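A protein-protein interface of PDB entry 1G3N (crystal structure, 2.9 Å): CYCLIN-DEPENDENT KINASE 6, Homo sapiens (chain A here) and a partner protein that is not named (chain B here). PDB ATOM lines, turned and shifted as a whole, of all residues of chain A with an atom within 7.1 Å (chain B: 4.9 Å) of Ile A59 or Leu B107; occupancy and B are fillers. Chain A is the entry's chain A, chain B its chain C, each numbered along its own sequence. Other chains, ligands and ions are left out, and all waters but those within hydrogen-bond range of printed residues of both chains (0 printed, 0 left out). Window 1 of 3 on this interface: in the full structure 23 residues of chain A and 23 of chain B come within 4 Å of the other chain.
O of Leu B107 sits at hydrogen-bond distance from NH1 of Arg A60 (3.5 Å).
NZ of Lys B106 sits at hydrogen-bond distance from O of Met A54, at 3.2 Å.
NH1 of Arg A60 is in hydrogen-bond range of O of Lys B106, at 2.7 Å.
The backbone NH of Met A54 lies within hydrogen-bond range of the side-chain carboxylate of Glu B135 (3.2 Å).
Glu B135 touches Gly A53.
CE of Met A54 touches CD1 of Leu B139 (3.7 Å).
Leu A56 touches Lys B106 (CD1 to NZ, 3.7 Å).
Trp B144 touches Thr A58 (CZ3 to CG2, 3.8 Å).
Ile A59 touches Lys B106.
Ile A59 touches Leu B107 (CG2 to CD2, 3.8 Å).
Ile A59 touches Glu B135 (CD1 to OE1, 3.8 Å).
CB of Ala A63 touches CD2 of Leu B107, at 3.8 Å.
Trp B144 touches Ala A63.
Ala A63 touches Thr B146.
Hydrophobic or aromatic side chains of chain A within 4 Å of the printed part of chain B: Met A54, Leu A56, Ile A59, Val A62 and Ala A63.
Of the 13 printed residues of chain B, 6 touch a printed residue of chain A.
Hydrophobic or aromatic side chains of chain B that line the printed part of chain A: Leu B107, Leu B139 and Trp B144.
N of Trp B144 is in hydrogen-bond range of O of Leu B139, at 2.9 Å.
Printed residues of chain B within 4 Å of Met A54: Lys B106 (3.2 Å), Glu B135 (3.2 Å), Leu B139 (3.7 Å) and Trp B144 (3.6 Å).
Ile A59 touches just these residues of chain B: Lys B106 (3.8 Å), Leu B107 (3.8 Å) and Glu B135 (3.8 Å).
Glu A61 touches none of the printed residues of chain B.
Printed residues of chain A within 4 Å of Leu B139: Met A54 (3.7 Å).
The nearest residue of chain B that does not touch Ile A59 is Thr B146 (4.1 Å).
The nearest residue of chain A that does not touch Leu B107 is Leu A56 (5.6 Å).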
ATOM      1  N   VAL A  47       3.152  -4.962 -19.594  1.00  0.00           N
ATOM      2  CA  VAL A  47       3.300  -5.726 -18.356  1.00  0.00           C
ATOM      3  C   VAL A  47       3.614  -7.201 -18.604  1.00  0.00           C
ATOM      4  O   VAL A  47       2.907  -7.921 -19.322  1.00  0.00           O
ATOM      5  CB  VAL A  47       2.042  -5.621 -17.455  1.00  0.00           C
ATOM      6  CG1 VAL A  47       2.351  -6.175 -16.078  1.00  0.00           C
ATOM      7  CG2 VAL A  47       1.587  -4.179 -17.356  1.00  0.00           C
ATOM      8  N   GLY A  53       1.874 -14.577 -11.768  1.00  0.00           N
ATOM      9  CA  GLY A  53       0.772 -13.824 -12.329  1.00  0.00           C
ATOM     10  C   GLY A  53       1.085 -12.384 -12.659  1.00  0.00           C
ATOM     11  O   GLY A  53       2.061 -12.095 -13.332  1.00  0.00           O
ATOM     12  N   MET A  54       0.247 -11.472 -12.186  1.00  0.00           N
ATOM     13  CA  MET A  54       0.442 -10.066 -12.469  1.00  0.00           C
ATOM     14  C   MET A  54       1.395  -9.477 -11.442  1.00  0.00           C
ATOM     15  O   MET A  54       1.223  -9.666 -10.243  1.00  0.00           O
ATOM     16  CB  MET A  54      -0.889  -9.338 -12.412  1.00  0.00           C
ATOM     17  CG  MET A  54      -0.915  -8.059 -13.210  1.00  0.00           C
ATOM     18  SD  MET A  54      -1.007  -8.390 -15.004  1.00  0.00           S
ATOM     19  CE  MET A  54      -2.627  -8.908 -15.227  1.00  0.00           C
ATOM     20  N   PRO A  55       2.420  -8.751 -11.905  1.00  0.00           N
ATOM     21  CA  PRO A  55       3.422  -8.126 -11.041  1.00  0.00           C
ATOM     22  C   PRO A  55       2.865  -7.239  -9.925  1.00  0.00           C
ATOM     23  O   PRO A  55       2.105  -6.310 -10.178  1.00  0.00           O
ATOM     24  CB  PRO A  55       4.276  -7.351 -12.044  1.00  0.00           C
ATOM     25  CG  PRO A  55       4.205  -8.239 -13.244  1.00  0.00           C
ATOM     26  CD  PRO A  55       2.722  -8.449 -13.311  1.00  0.00           C
ATOM     27  N   LEU A  56       3.252  -7.536  -8.692  1.00  0.00           N
ATOM     28  CA  LEU A  56       2.829  -6.748  -7.553  1.00  0.00           C
ATOM     29  C   LEU A  56       2.732  -5.251  -7.793  1.00  0.00           C
ATOM     30  O   LEU A  56       1.650  -4.666  -7.678  1.00  0.00           O
ATOM     31  CB  LEU A  56       3.781  -6.933  -6.378  1.00  0.00           C
ATOM     32  CG  LEU A  56       3.731  -8.203  -5.554  1.00  0.00           C
ATOM     33  CD1 LEU A  56       4.011  -9.438  -6.388  1.00  0.00           C
ATOM     34  CD2 LEU A  56       4.742  -8.033  -4.468  1.00  0.00           C
ATOM     35  N   SER A  57       3.865  -4.625  -8.111  1.00  0.00           N
ATOM     36  CA  SER A  57       3.874  -3.176  -8.284  1.00  0.00           C
ATOM     37  C   SER A  57       2.871  -2.668  -9.303  1.00  0.00           C
ATOM     38  O   SER A  57       2.187  -1.659  -9.052  1.00  0.00           O
ATOM     39  CB  SER A  57       5.296  -2.647  -8.591  1.00  0.00           C
ATOM     40  OG  SER A  57       5.839  -3.160  -9.783  1.00  0.00           O
ATOM     41  N   THR A  58       2.760  -3.364 -10.432  1.00  0.00           N
ATOM     42  CA  THR A  58       1.818  -2.939 -11.453  1.00  0.00           C
ATOM     43  C   THR A  58       0.469  -2.852 -10.775  1.00  0.00           C
ATOM     44  O   THR A  58      -0.214  -1.828 -10.840  1.00  0.00           O
ATOM     45  CB  THR A  58       1.738  -3.933 -12.608  1.00  0.00           C
ATOM     46  OG1 THR A  58       3.023  -4.034 -13.220  1.00  0.00           O
ATOM     47  CG2 THR A  58       0.763  -3.467 -13.645  1.00  0.00           C
ATOM     48  N   ILE A  59       0.105  -3.920 -10.078  1.00  0.00           N
ATOM     49  CA  ILE A  59      -1.169  -3.945  -9.393  1.00  0.00           C
ATOM     50  C   ILE A  59      -1.252  -2.847  -8.355  1.00  0.00           C
ATOM     51  O   ILE A  59      -2.193  -2.065  -8.363  1.00  0.00           O
ATOM     52  CB  ILE A  59      -1.425  -5.264  -8.708  1.00  0.00           C
ATOM     53  CG1 ILE A  59      -1.504  -6.391  -9.742  1.00  0.00           C
ATOM     54  CG2 ILE A  59      -2.721  -5.186  -7.978  1.00  0.00           C
ATOM     55  CD1 ILE A  59      -1.977  -7.756  -9.182  1.00  0.00           C
ATOM     56  N   ARG A  60      -0.259  -2.769  -7.479  1.00  0.00           N
ATOM     57  CA  ARG A  60      -0.264  -1.750  -6.435  1.00  0.00           C
ATOM     58  C   ARG A  60      -0.382  -0.331  -6.967  1.00  0.00           C
ATOM     59  O   ARG A  60      -1.149   0.481  -6.448  1.00  0.00           O
ATOM     60  CB  ARG A  60       1.000  -1.823  -5.573  1.00  0.00           C
ATOM     61  CG  ARG A  60       1.234  -3.118  -4.817  1.00  0.00           C
ATOM     62  CD  ARG A  60       2.510  -2.977  -4.016  1.00  0.00           C
ATOM     63  NE  ARG A  60       3.044  -4.252  -3.540  1.00  0.00           N
ATOM     64  CZ  ARG A  60       2.513  -4.972  -2.560  1.00  0.00           C
ATOM     65  NH1 ARG A  60       1.420  -4.534  -1.945  1.00  0.00           N
ATOM     66  NH2 ARG A  60       3.071  -6.127  -2.198  1.00  0.00           N
ATOM     67  N   GLU A  61       0.371  -0.020  -8.012  1.00  0.00           N
ATOM     68  CA  GLU A  61       0.358   1.342  -8.521  1.00  0.00           C
ATOM     69  C   GLU A  61      -0.978   1.758  -9.117  1.00  0.00           C
ATOM     70  O   GLU A  61      -1.484   2.869  -8.860  1.00  0.00           O
ATOM     71  CB  GLU A  61       1.504   1.500  -9.513  1.00  0.00           C
ATOM     72  CG  GLU A  61       2.862   1.199  -8.872  1.00  0.00           C
ATOM     73  CD  GLU A  61       4.033   1.333  -9.832  1.00  0.00           C
ATOM     74  OE1 GLU A  61       4.147   0.503 -10.778  1.00  0.00           O
ATOM     75  OE2 GLU A  61       4.836   2.280  -9.641  1.00  0.00           O
ATOM     76  N   VAL A  62      -1.556   0.860  -9.908  1.00  0.00           N
ATOM     77  CA  VAL A  62      -2.846   1.159 -10.527  1.00  0.00           C
ATOM     78  C   VAL A  62      -3.899   1.237  -9.445  1.00  0.00           C
ATOM     79  O   VAL A  62      -4.821   2.048  -9.525  1.00  0.00           O
ATOM     80  CB  VAL A  62      -3.285   0.096 -11.568  1.00  0.00           C
ATOM     81  CG1 VAL A  62      -4.609   0.508 -12.159  1.00  0.00           C
ATOM     82  CG2 VAL A  62      -2.254  -0.023 -12.691  1.00  0.00           C
ATOM     83  N   ALA A  63      -3.735   0.392  -8.429  1.00  0.00           N
ATOM     84  CA  ALA A  63      -4.641   0.328  -7.279  1.00  0.00           C
ATOM     85  C   ALA A  63      -4.720   1.680  -6.580  1.00  0.00           C
ATOM     86  O   ALA A  63      -5.816   2.217  -6.325  1.00  0.00           O
ATOM     87  CB  ALA A  63      -4.156  -0.729  -6.286  1.00  0.00           C
ATOM     88  N   VAL A  64      -3.548   2.224  -6.273  1.00  0.00           N
ATOM     89  CA  VAL A  64      -3.447   3.517  -5.599  1.00  0.00           C
ATOM     90  C   VAL A  64      -3.976   4.681  -6.449  1.00  0.00           C
ATOM     91  O   VAL A  64      -4.622   5.599  -5.946  1.00  0.00           O
ATOM     92  CB  VAL A  64      -1.974   3.799  -5.202  1.00  0.00           C
ATOM     93  CG1 VAL A  64      -1.831   5.197  -4.656  1.00  0.00           C
ATOM     94  CG2 VAL A  64      -1.516   2.768  -4.189  1.00  0.00           C
ATOM     95  N   LEU A  65      -3.688   4.653  -7.737  1.00  0.00           N
ATOM     96  CA  LEU A  65      -4.167   5.726  -8.577  1.00  0.00           C
ATOM     97  C   LEU A  65      -5.678   5.682  -8.572  1.00  0.00           C
ATOM     98  O   LEU A  65      -6.334   6.676  -8.263  1.00  0.00           O
ATOM     99  CB  LEU A  65      -3.612   5.584 -10.008  1.00  0.00           C
ATOM    100  CG  LEU A  65      -2.090   5.803 -10.076  1.00  0.00           C
ATOM    101  CD1 LEU A  65      -1.536   5.442 -11.458  1.00  0.00           C
ATOM    102  CD2 LEU A  65      -1.821   7.267  -9.689  1.00  0.00           C
ATOM    103  N   LEU A  94      -1.091  -2.495 -20.938  1.00  0.00           N
ATOM    104  CA  LEU A  94      -1.843  -1.733 -19.944  1.00  0.00           C
ATOM    105  C   LEU A  94      -1.853  -0.240 -20.299  1.00  0.00           C
ATOM    106  O   LEU A  94      -0.813   0.340 -20.606  1.00  0.00           O
ATOM    107  CB  LEU A  94      -1.204  -1.922 -18.573  1.00  0.00           C
ATOM    108  CG  LEU A  94      -2.148  -1.992 -17.375  1.00  0.00           C
ATOM    109  CD1 LEU A  94      -1.301  -1.872 -16.124  1.00  0.00           C
ATOM    110  CD2 LEU A  94      -3.187  -0.879 -17.403  1.00  0.00           C
ATOM    111  N   LEU B  74     -10.210  -7.513   2.578  1.00  0.00           N
ATOM    112  CA  LEU B  74     -10.133  -7.024   1.220  1.00  0.00           C
ATOM    113  C   LEU B  74     -10.515  -8.127   0.262  1.00  0.00           C
ATOM    114  O   LEU B  74     -11.350  -7.905  -0.622  1.00  0.00           O
ATOM    115  CB  LEU B  74      -8.732  -6.499   0.937  1.00  0.00           C
ATOM    116  CG  LEU B  74      -8.441  -5.826  -0.411  1.00  0.00           C
ATOM    117  CD1 LEU B  74      -9.454  -4.740  -0.705  1.00  0.00           C
ATOM    118  CD2 LEU B  74      -7.026  -5.251  -0.371  1.00  0.00           C
ATOM    119  N   VAL B 103      -4.779 -11.671  -5.284  1.00  0.00           N
ATOM    120  CA  VAL B 103      -4.762 -10.222  -5.440  1.00  0.00           C
ATOM    121  C   VAL B 103      -4.761  -9.493  -4.067  1.00  0.00           C
ATOM    122  O   VAL B 103      -3.919  -8.618  -3.832  1.00  0.00           O
ATOM    123  CB  VAL B 103      -5.983  -9.727  -6.300  1.00  0.00           C
ATOM    124  CG1 VAL B 103      -5.998  -8.200  -6.376  1.00  0.00           C
ATOM    125  CG2 VAL B 103      -5.920 -10.324  -7.692  1.00  0.00           C
ATOM    126  N   ALA B 104      -5.682  -9.852  -3.168  1.00  0.00           N
ATOM    127  CA  ALA B 104      -5.739  -9.193  -1.857  1.00  0.00           C
ATOM    128  C   ALA B 104      -4.419  -9.213  -1.098  1.00  0.00           C
ATOM    129  O   ALA B 104      -4.071  -8.217  -0.486  1.00  0.00           O
ATOM    130  CB  ALA B 104      -6.831  -9.788  -0.988  1.00  0.00           C
ATOM    131  N   SER B 105      -3.679 -10.320  -1.119  1.00  0.00           N
ATOM    132  CA  SER B 105      -2.412 -10.337  -0.401  1.00  0.00           C
ATOM    133  C   SER B 105      -1.321  -9.635  -1.201  1.00  0.00           C
ATOM    134  O   SER B 105      -0.391  -9.070  -0.624  1.00  0.00           O
ATOM    135  CB  SER B 105      -1.973 -11.767  -0.033  1.00  0.00           C
ATOM    136  OG  SER B 105      -1.702 -12.553  -1.169  1.00  0.00           O
ATOM    137  N   LYS B 106      -1.425  -9.654  -2.528  1.00  0.00           N
ATOM    138  CA  LYS B 106      -0.433  -8.955  -3.338  1.00  0.00           C
ATOM    139  C   LYS B 106      -0.518  -7.481  -2.998  1.00  0.00           C
ATOM    140  O   LYS B 106       0.450  -6.757  -3.176  1.00  0.00           O
ATOM    141  CB  LYS B 106      -0.686  -9.122  -4.840  1.00  0.00           C
ATOM    142  CG  LYS B 106      -0.194 -10.400  -5.467  1.00  0.00           C
ATOM    143  CD  LYS B 106      -0.664 -10.453  -6.892  1.00  0.00           C
ATOM    144  CE  LYS B 106      -0.183 -11.680  -7.624  1.00  0.00           C
ATOM    145  NZ  LYS B 106       1.310 -11.629  -7.681  1.00  0.00           N
ATOM    146  N   LEU B 107      -1.677  -7.051  -2.505  1.00  0.00           N
ATOM    147  CA  LEU B 107      -1.918  -5.658  -2.151  1.00  0.00           C
ATOM    148  C   LEU B 107      -1.739  -5.345  -0.687  1.00  0.00           C
ATOM    149  O   LEU B 107      -1.621  -4.174  -0.312  1.00  0.00           O
ATOM    150  CB  LEU B 107      -3.345  -5.245  -2.519  1.00  0.00           C
ATOM    151  CG  LEU B 107      -3.666  -4.930  -3.975  1.00  0.00           C
ATOM    152  CD1 LEU B 107      -5.143  -4.600  -4.145  1.00  0.00           C
ATOM    153  CD2 LEU B 107      -2.805  -3.766  -4.405  1.00  0.00           C
ATOM    154  N   ARG B 108      -1.728  -6.375   0.151  1.00  0.00           N
ATOM    155  CA  ARG B 108      -1.636  -6.125   1.575  1.00  0.00           C
ATOM    156  C   ARG B 108      -0.623  -6.895   2.400  1.00  0.00           C
ATOM    157  O   ARG B 108      -0.307  -6.452   3.498  1.00  0.00           O
ATOM    158  CB  ARG B 108      -3.006  -6.328   2.218  1.00  0.00           C
ATOM    159  CG  ARG B 108      -4.120  -5.448   1.714  1.00  0.00           C
ATOM    160  CD  ARG B 108      -3.799  -3.996   1.863  1.00  0.00           C
ATOM    161  NE  ARG B 108      -4.995  -3.197   1.647  1.00  0.00           N
ATOM    162  CZ  ARG B 108      -5.625  -2.538   2.608  1.00  0.00           C
ATOM    163  NH1 ARG B 108      -5.159  -2.585   3.843  1.00  0.00           N
ATOM    164  NH2 ARG B 108      -6.725  -1.839   2.340  1.00  0.00           N
ATOM    165  N   SER B 109      -0.114  -8.030   1.940  1.00  0.00           N
ATOM    166  CA  SER B 109       0.830  -8.725   2.811  1.00  0.00           C
ATOM    167  C   SER B 109       2.266  -8.570   2.386  1.00  0.00           C
ATOM    168  O   SER B 109       2.562  -8.458   1.188  1.00  0.00           O
ATOM    169  CB  SER B 109       0.477 -10.220   2.973  1.00  0.00           C
ATOM    170  OG  SER B 109       0.450 -10.935   1.752  1.00  0.00           O
ATOM    171  N   GLU B 135      -7.168 -14.256 -12.162  1.00  0.00           N
ATOM    172  CA  GLU B 135      -6.650 -13.024 -11.612  1.00  0.00           C
ATOM    173  C   GLU B 135      -6.769 -11.958 -12.686  1.00  0.00           C
ATOM    174  O   GLU B 135      -7.194 -10.842 -12.399  1.00  0.00           O
ATOM    175  CB  GLU B 135      -5.186 -13.153 -11.234  1.00  0.00           C
ATOM    176  CG  GLU B 135      -4.657 -11.977 -10.411  1.00  0.00           C
ATOM    177  CD  GLU B 135      -3.157 -12.061 -10.228  1.00  0.00           C
ATOM    178  OE1 GLU B 135      -2.628 -11.535  -9.219  1.00  0.00           O
ATOM    179  OE2 GLU B 135      -2.504 -12.649 -11.124  1.00  0.00           O
ATOM    180  N   LEU B 139      -9.184  -8.670 -12.441  1.00  0.00           N
ATOM    181  CA  LEU B 139      -8.670  -7.316 -12.635  1.00  0.00           C
ATOM    182  C   LEU B 139      -9.424  -6.594 -13.753  1.00  0.00           C
ATOM    183  O   LEU B 139      -9.724  -5.411 -13.667  1.00  0.00           O
ATOM    184  CB  LEU B 139      -7.159  -7.336 -12.910  1.00  0.00           C
ATOM    185  CG  LEU B 139      -6.197  -7.969 -11.867  1.00  0.00           C
ATOM    186  CD1 LEU B 139      -4.755  -7.885 -12.417  1.00  0.00           C
ATOM    187  CD2 LEU B 139      -6.274  -7.293 -10.500  1.00  0.00           C
ATOM    188  N   TRP B 144      -9.021  -2.835 -12.549  1.00  0.00           N
ATOM    189  CA  TRP B 144      -7.878  -2.567 -11.699  1.00  0.00           C
ATOM    190  C   TRP B 144      -8.122  -1.766 -10.440  1.00  0.00           C
ATOM    191  O   TRP B 144      -7.177  -1.352  -9.779  1.00  0.00           O
ATOM    192  CB  TRP B 144      -6.766  -1.948 -12.524  1.00  0.00           C
ATOM    193  CG  TRP B 144      -6.302  -2.887 -13.596  1.00  0.00           C
ATOM    194  CD1 TRP B 144      -7.003  -3.263 -14.712  1.00  0.00           C
ATOM    195  CD2 TRP B 144      -5.066  -3.622 -13.634  1.00  0.00           C
ATOM    196  NE1 TRP B 144      -6.281  -4.183 -15.437  1.00  0.00           N
ATOM    197  CE2 TRP B 144      -5.090  -4.421 -14.798  1.00  0.00           C
ATOM    198  CE3 TRP B 144      -3.945  -3.684 -12.800  1.00  0.00           C
ATOM    199  CZ2 TRP B 144      -4.034  -5.270 -15.147  1.00  0.00           C
ATOM    200  CZ3 TRP B 144      -2.894  -4.534 -13.154  1.00  0.00           C
ATOM    201  CH2 TRP B 144      -2.952  -5.310 -14.314  1.00  0.00           C
ATOM    202  N   THR B 146      -8.676  -2.281  -7.261  1.00  0.00           N
ATOM    203  CA  THR B 146      -8.568  -3.341  -6.293  1.00  0.00           C
ATOM    204  C   THR B 146      -8.445  -2.954  -4.853  1.00  0.00           C
ATOM    205  O   THR B 146      -8.531  -3.819  -3.971  1.00  0.00           O
ATOM    206  CB  THR B 146      -7.423  -4.245  -6.670  1.00  0.00           C
ATOM    207  OG1 THR B 146      -6.252  -3.449  -6.888  1.00  0.00           O
ATOM    208  CG2 THR B 146      -7.767  -5.001  -7.947  1.00  0.00           C
ATOM    209  N   GLU B 147      -8.230  -1.671  -4.593  1.00  0.00           N
ATOM    210  CA  GLU B 147      -8.178  -1.190  -3.209  1.00  0.00           C
ATOM    211  C   GLU B 147      -9.560  -0.675  -2.758  1.00  0.00           C
ATOM    212  O   GLU B 147     -10.383  -0.231  -3.585  1.00  0.00           O
ATOM    213  CB  GLU B 147      -7.166  -0.057  -3.045  1.00  0.00           C
ATOM    214  CG  GLU B 147      -5.784  -0.468  -2.601  1.00  0.00           C
ATOM    215  CD  GLU B 147      -5.754  -1.159  -1.241  1.00  0.00           C
ATOM    216  OE1 GLU B 147      -6.644  -0.897  -0.380  1.00  0.00           O
ATOM    217  OE2 GLU B 147      -4.801  -1.950  -1.031  1.00  0.00           O
